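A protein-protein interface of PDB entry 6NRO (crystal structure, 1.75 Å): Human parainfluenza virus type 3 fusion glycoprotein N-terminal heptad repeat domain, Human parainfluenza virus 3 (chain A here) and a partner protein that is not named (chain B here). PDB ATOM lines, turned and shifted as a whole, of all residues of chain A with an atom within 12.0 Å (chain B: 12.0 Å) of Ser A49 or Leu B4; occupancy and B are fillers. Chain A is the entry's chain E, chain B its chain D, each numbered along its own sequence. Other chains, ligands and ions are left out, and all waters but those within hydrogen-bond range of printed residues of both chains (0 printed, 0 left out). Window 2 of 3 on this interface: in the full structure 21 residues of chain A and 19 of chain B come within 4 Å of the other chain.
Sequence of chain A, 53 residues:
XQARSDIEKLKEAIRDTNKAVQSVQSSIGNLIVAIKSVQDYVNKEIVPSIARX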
ATOM      1  N   SER A  37      -8.633 -21.067 -11.913  1.00  0.00           N
ATOM      2  CA  SER A  37      -9.008 -21.666 -13.191  1.00  0.00           C
ATOM      3  C   SER A  37      -8.989 -23.180 -13.101  1.00  0.00           C
ATOM      4  O   SER A  37      -9.849 -23.856 -13.672  1.00  0.00           O
ATOM      5  CB  SER A  37      -8.070 -21.208 -14.301  1.00  0.00           C
ATOM      6  OG  SER A  37      -7.972 -19.802 -14.310  1.00  0.00           O
ATOM      7  N   VAL A  38      -8.009 -23.734 -12.389  1.00  0.00           N
ATOM      8  CA  VAL A  38      -7.985 -25.180 -12.216  1.00  0.00           C
ATOM      9  C   VAL A  38      -9.201 -25.640 -11.421  1.00  0.00           C
ATOM     10  O   VAL A  38      -9.830 -26.644 -11.764  1.00  0.00           O
ATOM     11  CB  VAL A  38      -6.680 -25.623 -11.544  1.00  0.00           C
ATOM     12  CG1 VAL A  38      -6.723 -27.133 -11.296  1.00  0.00           C
ATOM     13  CG2 VAL A  38      -5.490 -25.198 -12.395  1.00  0.00           C
ATOM     14  N   GLN A  39      -9.522 -24.939 -10.324  1.00  0.00           N
ATOM     15  CA  GLN A  39     -10.729 -25.254  -9.561  1.00  0.00           C
ATOM     16  C   GLN A  39     -11.962 -25.237 -10.455  1.00  0.00           C
ATOM     17  O   GLN A  39     -12.754 -26.184 -10.463  1.00  0.00           O
ATOM     18  CB  GLN A  39     -10.897 -24.261  -8.408  1.00  0.00           C
ATOM     19  CG  GLN A  39     -12.116 -24.493  -7.527  1.00  0.00           C
ATOM     20  CD  GLN A  39     -12.388 -23.308  -6.613  1.00  0.00           C
ATOM     21  OE1 GLN A  39     -12.399 -23.437  -5.391  1.00  0.00           O
ATOM     22  NE2 GLN A  39     -12.612 -22.146  -7.206  1.00  0.00           N
ATOM     23  N   ASP A  40     -12.134 -24.169 -11.231  1.00  0.00           N
ATOM     24  CA  ASP A  40     -13.328 -24.052 -12.058  1.00  0.00           C
ATOM     25  C   ASP A  40     -13.364 -25.131 -13.134  1.00  0.00           C
ATOM     26  O   ASP A  40     -14.428 -25.688 -13.428  1.00  0.00           O
ATOM     27  CB  ASP A  40     -13.385 -22.656 -12.673  1.00  0.00           C
ATOM     28  CG  ASP A  40     -13.606 -21.575 -11.630  1.00  0.00           C
ATOM     29  OD1 ASP A  40     -13.979 -21.897 -10.480  1.00  0.00           O
ATOM     30  OD2 ASP A  40     -13.409 -20.388 -11.964  1.00  0.00           O
ATOM     31  N   TYR A  41     -12.209 -25.457 -13.719  1.00  0.00           N
ATOM     32  CA  TYR A  41     -12.181 -26.510 -14.727  1.00  0.00           C
ATOM     33  C   TYR A  41     -12.580 -27.845 -14.123  1.00  0.00           C
ATOM     34  O   TYR A  41     -13.321 -28.617 -14.743  1.00  0.00           O
ATOM     35  CB  TYR A  41     -10.793 -26.609 -15.347  1.00  0.00           C
ATOM     36  CG  TYR A  41     -10.649 -27.704 -16.371  1.00  0.00           C
ATOM     37  CD1 TYR A  41     -10.792 -27.433 -17.725  1.00  0.00           C
ATOM     38  CD2 TYR A  41     -10.364 -29.010 -15.987  1.00  0.00           C
ATOM     39  CE1 TYR A  41     -10.655 -28.435 -18.669  1.00  0.00           C
ATOM     40  CE2 TYR A  41     -10.228 -30.010 -16.920  1.00  0.00           C
ATOM     41  CZ  TYR A  41     -10.371 -29.719 -18.254  1.00  0.00           C
ATOM     42  OH  TYR A  41     -10.227 -30.718 -19.175  1.00  0.00           O
ATOM     43  N   VAL A  42     -12.092 -28.141 -12.915  1.00  0.00           N
ATOM     44  CA  VAL A  42     -12.456 -29.388 -12.250  1.00  0.00           C
ATOM     45  C   VAL A  42     -13.958 -29.433 -12.021  1.00  0.00           C
ATOM     46  O   VAL A  42     -14.630 -30.412 -12.367  1.00  0.00           O
ATOM     47  CB  VAL A  42     -11.671 -29.548 -10.933  1.00  0.00           C
ATOM     48  CG1 VAL A  42     -12.267 -30.676 -10.099  1.00  0.00           C
ATOM     49  CG2 VAL A  42     -10.198 -29.810 -11.223  1.00  0.00           C
ATOM     50  N   ASN A  43     -14.513 -28.351 -11.495  1.00  0.00           N
ATOM     51  CA  ASN A  43     -15.946 -28.260 -11.129  1.00  0.00           C
ATOM     52  C   ASN A  43     -16.850 -28.250 -12.358  1.00  0.00           C
ATOM     53  O   ASN A  43     -17.872 -28.904 -12.319  1.00  0.00           O
ATOM     54  CB  ASN A  43     -16.219 -27.029 -10.284  1.00  0.00           C
ATOM     55  CG  ASN A  43     -15.711 -27.214  -8.882  1.00  0.00           C
ATOM     56  OD1 ASN A  43     -15.464 -28.330  -8.479  1.00  0.00           O
ATOM     57  ND2 ASN A  43     -15.544 -26.136  -8.153  1.00  0.00           N
ATOM     58  N   LYS A  44     -16.466 -27.550 -13.408  1.00  0.00           N
ATOM     59  CA  LYS A  44     -17.317 -27.381 -14.603  1.00  0.00           C
ATOM     60  C   LYS A  44     -17.100 -28.499 -15.620  1.00  0.00           C
ATOM     61  O   LYS A  44     -18.072 -28.879 -16.226  1.00  0.00           O
ATOM     62  CB  LYS A  44     -17.068 -26.001 -15.214  1.00  0.00           C
ATOM     63  CG  LYS A  44     -17.399 -24.825 -14.304  1.00  0.00           C
ATOM     64  N   GLU A  45     -15.895 -29.021 -15.802  1.00  0.00           N
ATOM     65  CA  GLU A  45     -15.661 -30.032 -16.856  1.00  0.00           C
ATOM     66  C   GLU A  45     -15.488 -31.440 -16.308  1.00  0.00           C
ATOM     67  O   GLU A  45     -15.954 -32.357 -16.950  1.00  0.00           O
ATOM     68  CB  GLU A  45     -14.394 -29.744 -17.655  1.00  0.00           C
ATOM     69  CG  GLU A  45     -14.317 -28.339 -18.191  1.00  0.00           C
ATOM     70  CD  GLU A  45     -15.325 -28.023 -19.269  1.00  0.00           C
ATOM     71  OE1 GLU A  45     -15.744 -28.932 -19.962  1.00  0.00           O
ATOM     72  OE2 GLU A  45     -15.677 -26.876 -19.399  1.00  0.00           O
ATOM     73  N   ILE A  46     -14.809 -31.617 -15.192  1.00  0.00           N
ATOM     74  CA  ILE A  46     -14.494 -32.987 -14.727  1.00  0.00           C
ATOM     75  C   ILE A  46     -15.620 -33.566 -13.888  1.00  0.00           C
ATOM     76  O   ILE A  46     -15.993 -34.684 -14.144  1.00  0.00           O
ATOM     77  CB  ILE A  46     -13.178 -33.019 -13.941  1.00  0.00           C
ATOM     78  CG1 ILE A  46     -11.992 -32.610 -14.805  1.00  0.00           C
ATOM     79  CG2 ILE A  46     -12.972 -34.388 -13.336  1.00  0.00           C
ATOM     80  CD1 ILE A  46     -10.731 -32.468 -14.016  1.00  0.00           C
ATOM     81  N   VAL A  47     -16.089 -32.854 -12.880  1.00  0.00           N
ATOM     82  CA  VAL A  47     -17.102 -33.407 -11.983  1.00  0.00           C
ATOM     83  C   VAL A  47     -18.367 -33.775 -12.736  1.00  0.00           C
ATOM     84  O   VAL A  47     -18.851 -34.909 -12.571  1.00  0.00           O
ATOM     85  CB  VAL A  47     -17.372 -32.426 -10.821  1.00  0.00           C
ATOM     86  CG1 VAL A  47     -18.648 -32.822 -10.077  1.00  0.00           C
ATOM     87  CG2 VAL A  47     -16.175 -32.388  -9.863  1.00  0.00           C
ATOM     88  N   PRO A  48     -18.975 -32.889 -13.527  1.00  0.00           N
ATOM     89  CA  PRO A  48     -20.119 -33.328 -14.351  1.00  0.00           C
ATOM     90  C   PRO A  48     -19.841 -34.604 -15.138  1.00  0.00           C
ATOM     91  O   PRO A  48     -20.661 -35.529 -15.126  1.00  0.00           O
ATOM     92  CB  PRO A  48     -20.358 -32.124 -15.273  1.00  0.00           C
ATOM     93  CG  PRO A  48     -19.745 -30.929 -14.568  1.00  0.00           C
ATOM     94  CD  PRO A  48     -18.886 -31.423 -13.426  1.00  0.00           C
ATOM     95  N   SER A  49     -18.732 -34.657 -15.855  1.00  0.00           N
ATOM     96  CA  SER A  49     -18.364 -35.843 -16.655  1.00  0.00           C
ATOM     97  C   SER A  49     -18.386 -37.079 -15.759  1.00  0.00           C
ATOM     98  O   SER A  49     -18.943 -38.087 -16.155  1.00  0.00           O
ATOM     99  CB  SER A  49     -17.026 -35.680 -17.286  1.00  0.00           C
ATOM    100  OG  SER A  49     -17.116 -34.937 -18.484  1.00  0.00           O
ATOM    101  N   ILE A  50     -17.798 -36.979 -14.576  1.00  0.00           N
ATOM    102  CA  ILE A  50     -17.642 -38.127 -13.644  1.00  0.00           C
ATOM    103  C   ILE A  50     -18.989 -38.508 -13.022  1.00  0.00           C
ATOM    104  O   ILE A  50     -19.147 -39.689 -12.714  1.00  0.00           O
ATOM    105  CB  ILE A  50     -16.582 -37.815 -12.582  1.00  0.00           C
ATOM    106  CG1 ILE A  50     -15.213 -38.325 -13.011  1.00  0.00           C
ATOM    107  CG2 ILE A  50     -16.988 -38.372 -11.237  1.00  0.00           C
ATOM    108  CD1 ILE A  50     -14.123 -37.941 -12.071  1.00  0.00           C
ATOM    109  N   ALA A  51     -19.896 -37.546 -12.858  1.00  0.00           N
ATOM    110  CA  ALA A  51     -21.248 -37.720 -12.279  1.00  0.00           C
ATOM    111  C   ALA A  51     -22.123 -38.531 -13.240  1.00  0.00           C
ATOM    112  O   ALA A  51     -23.078 -39.168 -12.781  1.00  0.00           O
ATOM    113  CB  ALA A  51     -21.854 -36.370 -12.021  1.00  0.00           C
ATOM    114  N   ARG A  52     -21.815 -38.439 -14.534  1.00  0.00           N
ATOM    115  CA  ARG A  52     -22.507 -39.135 -15.642  1.00  0.00           C
ATOM    116  C   ARG A  52     -21.723 -40.397 -15.977  1.00  0.00           C
ATOM    117  O   ARG A  52     -22.053 -41.435 -15.396  1.00  0.00           O
ATOM    118  CB  ARG A  52     -22.602 -38.215 -16.861  1.00  0.00           C
ATOM    119  N   LEU B   4     -12.327 -34.422 -23.699  1.00  0.00           N
ATOM    120  CA  LEU B   4     -12.646 -33.071 -23.191  1.00  0.00           C
ATOM    121  C   LEU B   4     -11.506 -32.147 -23.629  1.00  0.00           C
ATOM    122  O   LEU B   4     -10.390 -32.641 -23.821  1.00  0.00           O
ATOM    123  CB  LEU B   4     -12.714 -33.126 -21.665  1.00  0.00           C
ATOM    124  CG  LEU B   4     -14.096 -32.970 -21.046  1.00  0.00           C
ATOM    125  CD1 LEU B   4     -13.985 -32.710 -19.557  1.00  0.00           C
ATOM    126  CD2 LEU B   4     -14.871 -31.860 -21.726  1.00  0.00           C
ATOM    127  N   ASP B   5     -11.762 -30.859 -23.790  1.00  0.00           N
ATOM    128  CA  ASP B   5     -10.679 -29.902 -24.109  1.00  0.00           C
ATOM    129  C   ASP B   5      -9.780 -29.853 -22.874  1.00  0.00           C
ATOM    130  O   ASP B   5     -10.298 -29.817 -21.773  1.00  0.00           O
ATOM    131  CB  ASP B   5     -11.228 -28.529 -24.476  1.00  0.00           C
ATOM    132  CG  ASP B   5     -11.590 -28.372 -25.936  1.00  0.00           C
ATOM    133  OD1 ASP B   5     -11.311 -29.275 -26.703  1.00  0.00           O
ATOM    134  OD2 ASP B   5     -12.159 -27.343 -26.273  1.00  0.00           O
ATOM    135  N   PRO B   6      -8.449 -29.882 -23.013  1.00  0.00           N
ATOM    136  CA  PRO B   6      -7.554 -29.819 -21.849  1.00  0.00           C
ATOM    137  C   PRO B   6      -7.628 -28.469 -21.159  1.00  0.00           C
ATOM    138  O   PRO B   6      -7.937 -27.447 -21.773  1.00  0.00           O
ATOM    139  CB  PRO B   6      -6.158 -30.057 -22.447  1.00  0.00           C
ATOM    140  CG  PRO B   6      -6.276 -29.583 -23.903  1.00  0.00           C
ATOM    141  CD  PRO B   6      -7.714 -29.938 -24.298  1.00  0.00           C
ATOM    142  N   ILE B   7      -7.333 -28.473 -19.861  1.00  0.00           N
ATOM    143  CA  ILE B   7      -7.121 -27.216 -19.156  1.00  0.00           C
ATOM    144  C   ILE B   7      -5.851 -26.573 -19.699  1.00  0.00           C
ATOM    145  O   ILE B   7      -4.847 -27.252 -19.941  1.00  0.00           O
ATOM    146  CB  ILE B   7      -7.022 -27.445 -17.642  1.00  0.00           C
ATOM    147  CG1 ILE B   7      -6.851 -26.104 -16.930  1.00  0.00           C
ATOM    148  CG2 ILE B   7      -5.867 -28.372 -17.327  1.00  0.00           C
ATOM    149  CD1 ILE B   7      -6.870 -26.198 -15.426  1.00  0.00           C
ATOM    150  N   ASP B   8      -5.889 -25.257 -19.899  1.00  0.00           N
ATOM    151  CA  ASP B   8      -4.763 -24.536 -20.485  1.00  0.00           C
ATOM    152  C   ASP B   8      -4.623 -23.221 -19.727  1.00  0.00           C
ATOM    153  O   ASP B   8      -5.334 -22.252 -20.011  1.00  0.00           O
ATOM    154  CB  ASP B   8      -4.944 -24.289 -21.977  1.00  0.00           C
ATOM    155  CG  ASP B   8      -3.682 -23.742 -22.623  1.00  0.00           C
ATOM    156  OD1 ASP B   8      -2.909 -23.065 -21.920  1.00  0.00           O
ATOM    157  OD2 ASP B   8      -3.454 -23.993 -23.820  1.00  0.00           O
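Of the 5 printed residues of chain B, 4 touch a printed residue of chain A.
Hydrophobic or aromatic side chains of chain B within 4 Å of the printed part of chain A: Leu B4 and Ile B7.
Of the 16 printed residues of chain A, 4 touch a printed residue of chain B.
Printed residues of chain A that touch a printed residue of chain B: Val A38, Tyr A41, Glu A45 and Ser A49.
Among the printed residues, 6 pairs touch across the chains.
The side-chain hydroxyl (OH) of Tyr A41 sits at hydrogen-bond distance from the backbone carbonyl oxygen (O) of Asp B5, at 2.8 Å.
O of Glu A45 lies within hydrogen-bond range of OG of Ser A49 (3.2 Å).
The backbone carbonyl oxygen (O) of Tyr A41 sits at hydrogen-bond distance from the backbone NH (N) of Ile A46, at 3.4 Å.
Of the printed residues of chain B, Val A38 touches Ile B7.
Of the printed residues of chain B, Tyr A41 touches Asp B5, Pro B6 and Ile B7.
Asn A43 touches none of the printed residues of chain B.
Of the printed residues of chain B, Glu A45 touches Leu B4 (3.3 Å).
No residue of chain B comes within 4 Å of Ile A46.
Pro A48 touches none of the printed residues of chain B.
Of the printed residues of chain B, Ser A49 touches Leu B4.
No residue of chain B comes within 4 Å of Ala A51.
No residue of chain B comes within 4 Å of Arg A52.
Of chain A, only Tyr A41 comes within 4 Å of Asp B5.
Of chain A, only Tyr A41 comes within 4 Å of Pro B6.
Of the printed residues of chain A, Ile B7 touches Val A38 and Tyr A41.
The nearest printed residue of chain A that does not touch Leu B4 is Tyr A41 (4.3 Å).
Among the printed residues, pairs that only touch across the chains: Val A38 with Ile B7, Tyr A41 with Pro B6, Tyr A41 with Ile B7, Glu A45 with Leu B4 and Ser A49 with Leu B4.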
